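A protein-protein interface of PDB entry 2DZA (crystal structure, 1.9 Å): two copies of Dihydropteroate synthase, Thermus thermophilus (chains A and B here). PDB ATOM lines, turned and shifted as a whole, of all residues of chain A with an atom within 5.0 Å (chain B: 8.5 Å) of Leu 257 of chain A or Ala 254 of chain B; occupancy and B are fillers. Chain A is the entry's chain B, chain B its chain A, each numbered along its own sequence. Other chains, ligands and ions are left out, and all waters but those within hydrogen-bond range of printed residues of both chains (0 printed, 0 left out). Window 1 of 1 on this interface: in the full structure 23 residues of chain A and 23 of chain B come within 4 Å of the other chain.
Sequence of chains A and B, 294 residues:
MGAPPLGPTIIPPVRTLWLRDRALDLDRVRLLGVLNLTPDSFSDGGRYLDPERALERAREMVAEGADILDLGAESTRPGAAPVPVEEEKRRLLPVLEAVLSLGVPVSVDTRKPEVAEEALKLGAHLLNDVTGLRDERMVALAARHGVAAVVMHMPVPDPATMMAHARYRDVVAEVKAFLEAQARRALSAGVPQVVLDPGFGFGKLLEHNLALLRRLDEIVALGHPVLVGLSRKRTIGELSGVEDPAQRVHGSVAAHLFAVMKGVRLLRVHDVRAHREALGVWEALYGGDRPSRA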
ATOM      1  N   SER A 252       2.159  -7.681 -10.337  1.00  0.00           N
ATOM      2  CA  SER A 252       3.158  -7.351  -9.317  1.00  0.00           C
ATOM      3  C   SER A 252       2.489  -6.796  -8.052  1.00  0.00           C
ATOM      4  O   SER A 252       2.835  -7.177  -6.930  1.00  0.00           O
ATOM      5  CB  SER A 252       4.170  -6.335  -9.859  1.00  0.00           C
ATOM      6  OG  SER A 252       4.969  -6.911 -10.882  1.00  0.00           O
ATOM      7  N   VAL A 253       1.542  -5.884  -8.239  1.00  0.00           N
ATOM      8  CA  VAL A 253       0.810  -5.299  -7.112  1.00  0.00           C
ATOM      9  C   VAL A 253       0.066  -6.407  -6.363  1.00  0.00           C
ATOM     10  O   VAL A 253       0.047  -6.433  -5.128  1.00  0.00           O
ATOM     11  CB  VAL A 253      -0.208  -4.222  -7.605  1.00  0.00           C
ATOM     12  CG1 VAL A 253      -1.213  -3.879  -6.489  1.00  0.00           C
ATOM     13  CG2 VAL A 253       0.547  -2.956  -8.022  1.00  0.00           C
ATOM     14  N   ALA A 254      -0.537  -7.329  -7.109  1.00  0.00           N
ATOM     15  CA  ALA A 254      -1.266  -8.431  -6.494  1.00  0.00           C
ATOM     16  C   ALA A 254      -0.343  -9.297  -5.622  1.00  0.00           C
ATOM     17  O   ALA A 254      -0.685  -9.633  -4.487  1.00  0.00           O
ATOM     18  CB  ALA A 254      -1.929  -9.288  -7.572  1.00  0.00           C
ATOM     19  N   ALA A 255       0.827  -9.649  -6.152  1.00  0.00           N
ATOM     20  CA  ALA A 255       1.786 -10.465  -5.406  1.00  0.00           C
ATOM     21  C   ALA A 255       2.225  -9.748  -4.133  1.00  0.00           C
ATOM     22  O   ALA A 255       2.293 -10.348  -3.052  1.00  0.00           O
ATOM     23  CB  ALA A 255       3.009 -10.762  -6.280  1.00  0.00           C
ATOM     24  N   HIS A 256       2.531  -8.462  -4.273  1.00  0.00           N
ATOM     25  CA  HIS A 256       2.966  -7.647  -3.150  1.00  0.00           C
ATOM     26  C   HIS A 256       1.892  -7.467  -2.069  1.00  0.00           C
ATOM     27  O   HIS A 256       2.213  -7.446  -0.880  1.00  0.00           O
ATOM     28  CB  HIS A 256       3.459  -6.298  -3.671  1.00  0.00           C
ATOM     29  CG  HIS A 256       4.794  -6.382  -4.348  1.00  0.00           C
ATOM     30  ND1 HIS A 256       5.244  -5.430  -5.237  1.00  0.00           N
ATOM     31  CD2 HIS A 256       5.785  -7.301  -4.248  1.00  0.00           C
ATOM     32  CE1 HIS A 256       6.454  -5.758  -5.655  1.00  0.00           C
ATOM     33  NE2 HIS A 256       6.807  -6.890  -5.070  1.00  0.00           N
ATOM     34  N   LEU A 257       0.629  -7.343  -2.471  1.00  0.00           N
ATOM     35  CA  LEU A 257      -0.446  -7.203  -1.485  1.00  0.00           C
ATOM     36  C   LEU A 257      -0.552  -8.513  -0.711  1.00  0.00           C
ATOM     37  O   LEU A 257      -0.797  -8.520   0.500  1.00  0.00           O
ATOM     38  CB  LEU A 257      -1.775  -6.866  -2.176  1.00  0.00           C
ATOM     39  CG  LEU A 257      -1.822  -5.446  -2.762  1.00  0.00           C
ATOM     40  CD1 LEU A 257      -3.173  -5.181  -3.418  1.00  0.00           C
ATOM     41  CD2 LEU A 257      -1.554  -4.428  -1.645  1.00  0.00           C
ATOM     42  N   PHE A 258      -0.364  -9.628  -1.410  1.00  0.00           N
ATOM     43  CA  PHE A 258      -0.399 -10.932  -0.758  1.00  0.00           C
ATOM     44  C   PHE A 258       0.737 -10.995   0.264  1.00  0.00           C
ATOM     45  O   PHE A 258       0.544 -11.463   1.388  1.00  0.00           O
ATOM     46  CB  PHE A 258      -0.259 -12.051  -1.800  1.00  0.00           C
ATOM     47  CG  PHE A 258      -0.375 -13.437  -1.223  1.00  0.00           C
ATOM     48  CD1 PHE A 258       0.746 -14.099  -0.736  1.00  0.00           C
ATOM     49  CD2 PHE A 258      -1.611 -14.077  -1.163  1.00  0.00           C
ATOM     50  CE1 PHE A 258       0.639 -15.387  -0.192  1.00  0.00           C
ATOM     51  CE2 PHE A 258      -1.735 -15.360  -0.623  1.00  0.00           C
ATOM     52  CZ  PHE A 258      -0.604 -16.017  -0.136  1.00  0.00           C
ATOM     53  N   ALA A 259       1.920 -10.513  -0.115  1.00  0.00           N
ATOM     54  CA  ALA A 259       3.067 -10.497   0.795  1.00  0.00           C
ATOM     55  C   ALA A 259       2.771  -9.602   2.006  1.00  0.00           C
ATOM     56  O   ALA A 259       3.119  -9.934   3.143  1.00  0.00           O
ATOM     57  CB  ALA A 259       4.309  -9.986   0.075  1.00  0.00           C
ATOM     58  N   VAL A 260       2.137  -8.462   1.761  1.00  0.00           N
ATOM     59  CA  VAL A 260       1.795  -7.557   2.856  1.00  0.00           C
ATOM     60  C   VAL A 260       0.831  -8.269   3.809  1.00  0.00           C
ATOM     61  O   VAL A 260       0.950  -8.159   5.035  1.00  0.00           O
ATOM     62  CB  VAL A 260       1.162  -6.251   2.318  1.00  0.00           C
ATOM     63  CG1 VAL A 260       0.521  -5.455   3.466  1.00  0.00           C
ATOM     64  CG2 VAL A 260       2.243  -5.409   1.655  1.00  0.00           C
ATOM     65  N   MET A 261      -0.110  -9.016   3.244  1.00  0.00           N
ATOM     66  CA  MET A 261      -1.073  -9.759   4.045  1.00  0.00           C
ATOM     67  C   MET A 261      -0.334 -10.791   4.900  1.00  0.00           C
ATOM     68  O   MET A 261      -0.782 -11.138   5.995  1.00  0.00           O
ATOM     69  CB  MET A 261      -2.084 -10.452   3.131  1.00  0.00           C
ATOM     70  CG  MET A 261      -3.105 -11.298   3.857  1.00  0.00           C
ATOM     71  SD  MET A 261      -4.286 -12.015   2.701  1.00  0.00           S
ATOM     72  CE  MET A 261      -3.360 -13.448   2.107  1.00  0.00           C
ATOM     73  N   ALA A 278      -2.531   1.418  -4.449  1.00  0.00           N
ATOM     74  CA  ALA A 278      -3.088   0.140  -4.003  1.00  0.00           C
ATOM     75  C   ALA A 278      -3.040   0.012  -2.478  1.00  0.00           C
ATOM     76  O   ALA A 278      -4.004  -0.444  -1.853  1.00  0.00           O
ATOM     77  CB  ALA A 278      -2.325  -1.035  -4.655  1.00  0.00           C
ATOM     78  N   LEU A 279      -1.916   0.415  -1.885  1.00  0.00           N
ATOM     79  CA  LEU A 279      -1.743   0.327  -0.435  1.00  0.00           C
ATOM     80  C   LEU A 279      -2.666   1.276   0.320  1.00  0.00           C
ATOM     81  O   LEU A 279      -3.055   1.001   1.459  1.00  0.00           O
ATOM     82  CB  LEU A 279      -0.284   0.610  -0.056  1.00  0.00           C
ATOM     83  CG  LEU A 279       0.727  -0.489  -0.408  1.00  0.00           C
ATOM     84  CD1 LEU A 279       2.147   0.022  -0.190  1.00  0.00           C
ATOM     85  CD2 LEU A 279       0.455  -1.726   0.451  1.00  0.00           C
ATOM     86  N   VAL A 281      -5.655   1.848  -0.352  1.00  0.00           N
ATOM     87  CA  VAL A 281      -6.889   1.089  -0.211  1.00  0.00           C
ATOM     88  C   VAL A 281      -6.669  -0.094   0.734  1.00  0.00           C
ATOM     89  O   VAL A 281      -7.363  -0.235   1.747  1.00  0.00           O
ATOM     90  CB  VAL A 281      -7.374   0.530  -1.580  1.00  0.00           C
ATOM     91  CG1 VAL A 281      -8.540  -0.433  -1.375  1.00  0.00           C
ATOM     92  CG2 VAL A 281      -7.800   1.662  -2.500  1.00  0.00           C
ATOM     93  N   TRP A 282      -5.687  -0.933   0.410  1.00  0.00           N
ATOM     94  CA  TRP A 282      -5.433  -2.128   1.206  1.00  0.00           C
ATOM     95  C   TRP A 282      -5.247  -1.897   2.698  1.00  0.00           C
ATOM     96  O   TRP A 282      -5.890  -2.558   3.518  1.00  0.00           O
ATOM     97  CB  TRP A 282      -4.225  -2.896   0.657  1.00  0.00           C
ATOM     98  CG  TRP A 282      -4.117  -4.279   1.225  1.00  0.00           C
ATOM     99  CD1 TRP A 282      -3.399  -4.668   2.321  1.00  0.00           C
ATOM    100  CD2 TRP A 282      -4.804  -5.448   0.759  1.00  0.00           C
ATOM    101  NE1 TRP A 282      -3.600  -6.009   2.566  1.00  0.00           N
ATOM    102  CE2 TRP A 282      -4.456  -6.510   1.622  1.00  0.00           C
ATOM    103  CE3 TRP A 282      -5.683  -5.698  -0.304  1.00  0.00           C
ATOM    104  CZ2 TRP A 282      -4.958  -7.808   1.454  1.00  0.00           C
ATOM    105  CZ3 TRP A 282      -6.182  -6.986  -0.473  1.00  0.00           C
ATOM    106  CH2 TRP A 282      -5.816  -8.024   0.405  1.00  0.00           C
ATOM    107  N   LEU B 213     -17.101  -3.265   3.548  1.00  0.00           N
ATOM    108  CA  LEU B 213     -15.995  -3.970   2.922  1.00  0.00           C
ATOM    109  C   LEU B 213     -15.258  -4.815   3.967  1.00  0.00           C
ATOM    110  O   LEU B 213     -14.929  -5.974   3.712  1.00  0.00           O
ATOM    111  CB  LEU B 213     -15.056  -2.959   2.239  1.00  0.00           C
ATOM    112  CG  LEU B 213     -14.162  -3.461   1.091  1.00  0.00           C
ATOM    113  CD1 LEU B 213     -14.961  -4.318   0.133  1.00  0.00           C
ATOM    114  CD2 LEU B 213     -13.567  -2.270   0.347  1.00  0.00           C
ATOM    115  N   LEU B 230     -16.564  -1.862  -7.235  1.00  0.00           N
ATOM    116  CA  LEU B 230     -15.954  -0.658  -6.689  1.00  0.00           C
ATOM    117  C   LEU B 230     -15.135   0.070  -7.741  1.00  0.00           C
ATOM    118  O   LEU B 230     -14.465   1.061  -7.443  1.00  0.00           O
ATOM    119  CB  LEU B 230     -15.079  -1.023  -5.489  1.00  0.00           C
ATOM    120  CG  LEU B 230     -15.879  -1.472  -4.260  1.00  0.00           C
ATOM    121  CD1 LEU B 230     -15.130  -2.553  -3.502  1.00  0.00           C
ATOM    122  CD2 LEU B 230     -16.148  -0.272  -3.383  1.00  0.00           C
ATOM    123  N   ILE B 236     -12.755   4.538  -3.724  1.00  0.00           N
ATOM    124  CA  ILE B 236     -11.418   4.266  -4.215  1.00  0.00           C
ATOM    125  C   ILE B 236     -10.635   5.568  -4.362  1.00  0.00           C
ATOM    126  O   ILE B 236      -9.470   5.647  -3.977  1.00  0.00           O
ATOM    127  CB  ILE B 236     -11.462   3.540  -5.564  1.00  0.00           C
ATOM    128  CG1 ILE B 236     -12.271   2.248  -5.427  1.00  0.00           C
ATOM    129  CG2 ILE B 236     -10.042   3.267  -6.043  1.00  0.00           C
ATOM    130  CD1 ILE B 236     -11.770   1.310  -4.329  1.00  0.00           C
ATOM    131  N   SER B 240      -7.219   6.008  -2.242  1.00  0.00           N
ATOM    132  CA  SER B 240      -5.994   5.974  -3.043  1.00  0.00           C
ATOM    133  C   SER B 240      -5.450   7.350  -3.409  1.00  0.00           C
ATOM    134  O   SER B 240      -4.342   7.462  -3.934  1.00  0.00           O
ATOM    135  CB  SER B 240      -6.222   5.167  -4.325  1.00  0.00           C
ATOM    136  OG  SER B 240      -7.069   5.853  -5.231  1.00  0.00           O
ATOM    137  N   ARG B 248      -8.306   5.273 -11.601  1.00  0.00           N
ATOM    138  CA  ARG B 248      -8.372   4.574 -10.314  1.00  0.00           C
ATOM    139  C   ARG B 248      -8.205   3.054 -10.382  1.00  0.00           C
ATOM    140  O   ARG B 248      -8.587   2.343  -9.445  1.00  0.00           O
ATOM    141  CB  ARG B 248      -9.708   4.906  -9.624  1.00  0.00           C
ATOM    142  CG  ARG B 248      -9.834   6.372  -9.198  1.00  0.00           C
ATOM    143  CD  ARG B 248     -11.240   6.747  -8.720  1.00  0.00           C
ATOM    144  NE  ARG B 248     -11.277   8.140  -8.269  1.00  0.00           N
ATOM    145  CZ  ARG B 248     -12.385   8.842  -8.039  1.00  0.00           C
ATOM    146  NH1 ARG B 248     -13.580   8.295  -8.215  1.00  0.00           N
ATOM    147  NH2 ARG B 248     -12.296  10.106  -7.626  1.00  0.00           N
ATOM    148  N   VAL B 249      -7.619   2.551 -11.461  1.00  0.00           N
ATOM    149  CA  VAL B 249      -7.468   1.106 -11.608  1.00  0.00           C
ATOM    150  C   VAL B 249      -6.726   0.394 -10.473  1.00  0.00           C
ATOM    151  O   VAL B 249      -7.177  -0.657 -10.002  1.00  0.00           O
ATOM    152  CB  VAL B 249      -6.781   0.734 -12.950  1.00  0.00           C
ATOM    153  CG1 VAL B 249      -5.306   1.149 -12.932  1.00  0.00           C
ATOM    154  CG2 VAL B 249      -6.920  -0.771 -13.203  1.00  0.00           C
ATOM    155  N   HIS B 250      -5.609   0.961 -10.021  1.00  0.00           N
ATOM    156  CA  HIS B 250      -4.808   0.316  -8.973  1.00  0.00           C
ATOM    157  C   HIS B 250      -5.551   0.211  -7.630  1.00  0.00           C
ATOM    158  O   HIS B 250      -5.489  -0.792  -6.932  1.00  0.00           O
ATOM    159  CB  HIS B 250      -3.520   1.122  -8.791  1.00  0.00           C
ATOM    160  CG  HIS B 250      -2.653   0.972 -10.014  1.00  0.00           C
ATOM    161  ND1 HIS B 250      -2.292  -0.229 -10.530  1.00  0.00           N
ATOM    162  CD2 HIS B 250      -2.090   1.981 -10.803  1.00  0.00           C
ATOM    163  CE1 HIS B 250      -1.532   0.051 -11.606  1.00  0.00           C
ATOM    164  NE2 HIS B 250      -1.394   1.367 -11.794  1.00  0.00           N
ATOM    165  N   GLY B 251      -6.268   1.262  -7.242  1.00  0.00           N
ATOM    166  CA  GLY B 251      -7.022   1.182  -6.005  1.00  0.00           C
ATOM    167  C   GLY B 251      -8.203   0.231  -6.167  1.00  0.00           C
ATOM    168  O   GLY B 251      -8.580  -0.477  -5.235  1.00  0.00           O
ATOM    169  N   SER B 252      -8.800   0.208  -7.354  1.00  0.00           N
ATOM    170  CA  SER B 252      -9.948  -0.660  -7.600  1.00  0.00           C
ATOM    171  C   SER B 252      -9.530  -2.131  -7.537  1.00  0.00           C
ATOM    172  O   SER B 252     -10.214  -2.963  -6.932  1.00  0.00           O
ATOM    173  CB  SER B 252     -10.579  -0.337  -8.960  1.00  0.00           C
ATOM    174  OG  SER B 252     -11.025   1.013  -8.998  1.00  0.00           O
ATOM    175  N   VAL B 253      -8.397  -2.447  -8.147  1.00  0.00           N
ATOM    176  CA  VAL B 253      -7.901  -3.817  -8.128  1.00  0.00           C
ATOM    177  C   VAL B 253      -7.642  -4.231  -6.682  1.00  0.00           C
ATOM    178  O   VAL B 253      -8.005  -5.332  -6.271  1.00  0.00           O
ATOM    179  CB  VAL B 253      -6.604  -3.945  -8.958  1.00  0.00           C
ATOM    180  CG1 VAL B 253      -5.927  -5.295  -8.688  1.00  0.00           C
ATOM    181  CG2 VAL B 253      -6.945  -3.818 -10.444  1.00  0.00           C
ATOM    182  N   ALA B 254      -7.026  -3.347  -5.902  1.00  0.00           N
ATOM    183  CA  ALA B 254      -6.740  -3.654  -4.502  1.00  0.00           C
ATOM    184  C   ALA B 254      -8.028  -3.929  -3.709  1.00  0.00           C
ATOM    185  O   ALA B 254      -8.108  -4.893  -2.940  1.00  0.00           O
ATOM    186  CB  ALA B 254      -5.952  -2.492  -3.861  1.00  0.00           C
ATOM    187  N   ALA B 255      -9.035  -3.077  -3.891  1.00  0.00           N
ATOM    188  CA  ALA B 255     -10.305  -3.256  -3.188  1.00  0.00           C
ATOM    189  C   ALA B 255     -10.974  -4.564  -3.601  1.00  0.00           C
ATOM    190  O   ALA B 255     -11.530  -5.279  -2.770  1.00  0.00           O
ATOM    191  CB  ALA B 255     -11.231  -2.095  -3.480  1.00  0.00           C
ATOM    192  N   HIS B 256     -10.927  -4.872  -4.890  1.00  0.00           N
ATOM    193  CA  HIS B 256     -11.534  -6.094  -5.382  1.00  0.00           C
ATOM    194  C   HIS B 256     -10.790  -7.343  -4.896  1.00  0.00           C
ATOM    195  O   HIS B 256     -11.422  -8.357  -4.592  1.00  0.00           O
ATOM    196  CB  HIS B 256     -11.636  -6.027  -6.907  1.00  0.00           C
ATOM    197  CG  HIS B 256     -12.728  -5.117  -7.383  1.00  0.00           C
ATOM    198  ND1 HIS B 256     -12.714  -4.509  -8.618  1.00  0.00           N
ATOM    199  CD2 HIS B 256     -13.881  -4.730  -6.784  1.00  0.00           C
ATOM    200  CE1 HIS B 256     -13.813  -3.787  -8.763  1.00  0.00           C
ATOM    201  NE2 HIS B 256     -14.538  -3.904  -7.666  1.00  0.00           N
ATOM    202  N   LEU B 257      -9.463  -7.277  -4.797  1.00  0.00           N
ATOM    203  CA  LEU B 257      -8.719  -8.431  -4.291  1.00  0.00           C
ATOM    204  C   LEU B 257      -9.095  -8.641  -2.822  1.00  0.00           C
ATOM    205  O   LEU B 257      -9.174  -9.770  -2.341  1.00  0.00           O
ATOM    206  CB  LEU B 257      -7.208  -8.213  -4.427  1.00  0.00           C
ATOM    207  CG  LEU B 257      -6.684  -8.274  -5.870  1.00  0.00           C
ATOM    208  CD1 LEU B 257      -5.177  -8.116  -5.866  1.00  0.00           C
ATOM    209  CD2 LEU B 257      -7.075  -9.618  -6.517  1.00  0.00           C
ATOM    210  N   PHE B 258      -9.328  -7.545  -2.104  1.00  0.00           N
ATOM    211  CA  PHE B 258      -9.721  -7.659  -0.703  1.00  0.00           C
ATOM    212  C   PHE B 258     -11.081  -8.355  -0.626  1.00  0.00           C
ATOM    213  O   PHE B 258     -11.301  -9.218   0.227  1.00  0.00           O
ATOM    214  CB  PHE B 258      -9.800  -6.276  -0.045  1.00  0.00           C
ATOM    215  CG  PHE B 258     -10.121  -6.332   1.418  1.00  0.00           C
ATOM    216  CD1 PHE B 258      -9.107  -6.499   2.356  1.00  0.00           C
ATOM    217  CD2 PHE B 258     -11.438  -6.268   1.859  1.00  0.00           C
ATOM    218  CE1 PHE B 258      -9.393  -6.604   3.713  1.00  0.00           C
ATOM    219  CE2 PHE B 258     -11.735  -6.372   3.216  1.00  0.00           C
ATOM    220  CZ  PHE B 258     -10.710  -6.541   4.142  1.00  0.00           C
ATOM    221  N   ALA B 259     -11.992  -7.979  -1.519  1.00  0.00           N
ATOM    222  CA  ALA B 259     -13.321  -8.589  -1.559  1.00  0.00           C
ATOM    223  C   ALA B 259     -13.211 -10.080  -1.900  1.00  0.00           C
ATOM    224  O   ALA B 259     -13.934 -10.913  -1.352  1.00  0.00           O
ATOM    225  CB  ALA B 259     -14.193  -7.887  -2.592  1.00  0.00           C
ATOM    226  N   VAL B 260     -12.310 -10.412  -2.815  1.00  0.00           N
ATOM    227  CA  VAL B 260     -12.113 -11.808  -3.204  1.00  0.00           C
ATOM    228  C   VAL B 260     -11.609 -12.598  -1.998  1.00  0.00           C
ATOM    229  O   VAL B 260     -12.030 -13.738  -1.752  1.00  0.00           O
ATOM    230  CB  VAL B 260     -11.107 -11.904  -4.371  1.00  0.00           C
ATOM    231  CG1 VAL B 260     -10.613 -13.351  -4.538  1.00  0.00           C
ATOM    232  CG2 VAL B 260     -11.781 -11.419  -5.650  1.00  0.00           C
ATOM    233  N   MET B 261     -10.716 -11.979  -1.235  1.00  0.00           N
ATOM    234  CA  MET B 261     -10.171 -12.608  -0.039  1.00  0.00           C
ATOM    235  C   MET B 261     -11.302 -12.863   0.965  1.00  0.00           C
ATOM    236  O   MET B 261     -11.276 -13.851   1.708  1.00  0.00           O
ATOM    237  CB  MET B 261      -9.103 -11.709   0.585  1.00  0.00           C
ATOM    238  CG  MET B 261      -8.375 -12.334   1.750  1.00  0.00           C
ATOM    239  SD  MET B 261      -7.128 -11.215   2.394  1.00  0.00           S
ATOM    240  CE  MET B 261      -8.193  -9.999   3.235  1.00  0.00           C
ATOM    241  N   ALA B 274      -6.729  -5.719 -16.508  1.00  0.00           N
ATOM    242  CA  ALA B 274      -6.015  -5.483 -15.253  1.00  0.00           C
ATOM    243  C   ALA B 274      -6.435  -6.468 -14.160  1.00  0.00           C
ATOM    244  O   ALA B 274      -5.593  -6.950 -13.393  1.00  0.00           O
ATOM    245  CB  ALA B 274      -6.240  -4.057 -14.776  1.00  0.00           C
ATOM    246  N   HIS B 275      -7.732  -6.760 -14.081  1.00  0.00           N
ATOM    247  CA  HIS B 275      -8.218  -7.701 -13.070  1.00  0.00           C
ATOM    248  C   HIS B 275      -7.836  -9.154 -13.392  1.00  0.00           C
ATOM    249  O   HIS B 275      -7.478  -9.919 -12.494  1.00  0.00           O
ATOM    250  CB  HIS B 275      -9.741  -7.573 -12.887  1.00  0.00           C
ATOM    251  CG  HIS B 275     -10.148  -6.368 -12.090  1.00  0.00           C
ATOM    252  ND1 HIS B 275     -10.196  -5.100 -12.628  1.00  0.00           N
ATOM    253  CD2 HIS B 275     -10.473  -6.235 -10.781  1.00  0.00           C
ATOM    254  CE1 HIS B 275     -10.531  -4.235 -11.685  1.00  0.00           C
ATOM    255  NE2 HIS B 275     -10.702  -4.897 -10.554  1.00  0.00           N
ATOM    256  N   ALA B 278      -4.211  -9.482 -12.353  1.00  0.00           N
ATOM    257  CA  ALA B 278      -4.060  -9.520 -10.898  1.00  0.00           C
ATOM    258  C   ALA B 278      -4.588 -10.836 -10.319  1.00  0.00           C
ATOM    259  O   ALA B 278      -3.972 -11.418  -9.422  1.00  0.00           O
ATOM    260  CB  ALA B 278      -4.795  -8.334 -10.256  1.00  0.00           C
ATOM    261  N   VAL B 281      -2.394 -14.007 -10.548  1.00  0.00           N
ATOM    262  CA  VAL B 281      -1.428 -14.130  -9.475  1.00  0.00           C
ATOM    263  C   VAL B 281      -2.127 -14.459  -8.156  1.00  0.00           C
ATOM    264  O   VAL B 281      -1.752 -15.408  -7.461  1.00  0.00           O
ATOM    265  CB  VAL B 281      -0.629 -12.824  -9.282  1.00  0.00           C
ATOM    266  CG1 VAL B 281       0.202 -12.907  -8.012  1.00  0.00           C
ATOM    267  CG2 VAL B 281       0.293 -12.580 -10.491  1.00  0.00           C
ATOM    268  N   TRP B 282      -3.150 -13.676  -7.817  1.00  0.00           N
ATOM    269  CA  TRP B 282      -3.853 -13.867  -6.552  1.00  0.00           C
ATOM    270  C   TRP B 282      -4.434 -15.263  -6.343  1.00  0.00           C
ATOM    271  O   TRP B 282      -4.207 -15.887  -5.299  1.00  0.00           O
ATOM    272  CB  TRP B 282      -4.956 -12.805  -6.392  1.00  0.00           C
ATOM    273  CG  TRP B 282      -5.542 -12.765  -5.004  1.00  0.00           C
ATOM    274  CD1 TRP B 282      -6.622 -13.463  -4.549  1.00  0.00           C
ATOM    275  CD2 TRP B 282      -5.034 -12.036  -3.883  1.00  0.00           C
ATOM    276  NE1 TRP B 282      -6.816 -13.219  -3.208  1.00  0.00           N
ATOM    277  CE2 TRP B 282      -5.850 -12.348  -2.774  1.00  0.00           C
ATOM    278  CE3 TRP B 282      -3.959 -11.154  -3.704  1.00  0.00           C
ATOM    279  CZ2 TRP B 282      -5.632 -11.804  -1.503  1.00  0.00           C
ATOM    280  CZ3 TRP B 282      -3.740 -10.610  -2.443  1.00  0.00           C
ATOM    281  CH2 TRP B 282      -4.574 -10.941  -1.356  1.00  0.00           C
ATOM    282  N   LEU B 285      -1.802 -17.951  -5.770  1.00  0.00           N
ATOM    283  CA  LEU B 285      -1.216 -17.827  -4.436  1.00  0.00           C
ATOM    284  C   LEU B 285      -2.194 -18.194  -3.332  1.00  0.00           C
ATOM    285  O   LEU B 285      -1.971 -19.139  -2.567  1.00  0.00           O
ATOM    286  CB  LEU B 285      -0.737 -16.393  -4.194  1.00  0.00           C
ATOM    287  CG  LEU B 285       0.455 -15.903  -5.009  1.00  0.00           C
ATOM    288  CD1 LEU B 285       0.713 -14.436  -4.721  1.00  0.00           C
ATOM    289  CD2 LEU B 285       1.674 -16.743  -4.656  1.00  0.00           C
ATOM    290  N   TYR B 286      -3.267 -17.416  -3.250  1.00  0.00           N
ATOM    291  CA  TYR B 286      -4.308 -17.607  -2.253  1.00  0.00           C
ATOM    292  C   TYR B 286      -5.201 -18.755  -2.702  1.00  0.00           C
ATOM    293  O   TYR B 286      -6.403 -18.575  -2.917  1.00  0.00           O
ATOM    294  CB  TYR B 286      -5.129 -16.321  -2.117  1.00  0.00           C
ATOM    295  CG  TYR B 286      -5.861 -16.177  -0.804  1.00  0.00           C
ATOM    296  CD1 TYR B 286      -6.848 -17.087  -0.425  1.00  0.00           C
ATOM    297  CD2 TYR B 286      -5.577 -15.117   0.057  1.00  0.00           C
ATOM    298  CE1 TYR B 286      -7.537 -16.944   0.776  1.00  0.00           C
ATOM    299  CE2 TYR B 286      -6.256 -14.964   1.261  1.00  0.00           C
ATOM    300  CZ  TYR B 286      -7.236 -15.879   1.616  1.00  0.00           C
ATOM    301  OH  TYR B 286      -7.918 -15.727   2.804  1.00  0.00           O
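SD of Met 261 of chain A lies close to SD of Met 261 of chain B (3.0 Å).
Printed residues of chain B that touch a printed residue of chain A: His 250, Gly 251, Ala 254, Ala 255, Leu 257, Phe 258, Met 261, Ala 278, Val 281, Trp 282, Leu 285 and Tyr 286.
Hydrophobic or aromatic side chains of chain B within 4 Å of the printed part of chain A: Ala 254, Ala 255, Leu 257, Phe 258, Met 261, Val 281, Trp 282, Leu 285 and Tyr 286.
Of the 14 printed residues of chain A, 8 touch a printed residue of chain B.
Printed residues of chain A that touch a printed residue of chain B: Ala 254, Ala 255, Leu 257, Phe 258, Met 261, Ala 278, Val 281 and Trp 282.
Hydrophobic or aromatic side chains of chain A within 4 Å of the printed part of chain B: Ala 254, Ala 255, Leu 257, Phe 258, Met 261, Ala 278, Val 281 and Trp 282.
Ala 254 of chain A touches Ala 278 of chain B.
O of Ala 254 of chain A touches CE3 of Trp 282 of chain B, at 3.7 Å.
Val 281 of chain B touches Ala 255 of chain A.
CD1 of Leu 257 of chain A touches CB of Ala 254 of chain B (3.9 Å).
Phe 258 of chain A touches Trp 282 of chain B.
Leu 285 of chain B touches Phe 258 of chain A (CD1 to CG, 3.8 Å).
His 250 of chain B touches Ala 278 of chain A (O to CA, 3.9 Å).
Val 281 of chain A touches Gly 251 of chain B (CG2 to O, 3.6 Å).
Met 261 of chain B touches Trp 282 of chain A.
CH2 of Trp 282 of chain B touches CH2 of Trp 282 of chain A, at 3.6 Å.
Ala 254 of chain A touches Leu 257 of chain B, and with the chains exchanged Leu 257 of chain A touches Ala 254 of chain B.
Ala 254 of chain A touches Ala 278 of chain B, and with the chains exchanged Ala 278 of chain A touches Ala 254 of chain B.
Met 261 of chain B touches its own counterpart, Met 261 of chain A.
Trp 282 of chain B touches its own counterpart, Trp 282 of chain A.
Positions printed for both chains: 252, 253, 254, 255, 256, 257, 258, 259, 260, 261, 278, 281 and 282.
Printed residues of chain B within 4 Å of Ala 255 of chain A: Val 281 (3.8 Å).
Of the printed residues of chain B, Leu 257 of chain A touches Ala 254.
Of the printed residues of chain B, Ala 278 of chain A touches His 250 (3.9 Å) and Ala 254 (3.5 Å).
Ser 252 of chain B touches none of the printed residues of chain A.
Val 253 of chain B touches none of the printed residues of chain A.
Of chain A, only Leu 257 (3.9 Å), Ala 278 (3.5 Å) and Trp 282 (3.7 Å) come within 4 Å of Ala 254 of chain B.
Printed residues of chain A within 4 Å of Ala 255 of chain B: Val 281 (3.7 Å).
Printed residues of chain A within 4 Å of Met 261 of chain B: Met 261 and Trp 282.
Printed residues of chain A within 4 Å of Val 281 of chain B: Ala 255.
The nearest residue of chain A that does not touch Ala 254 of chain B is Val 281 of chain A (4.04 Å).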
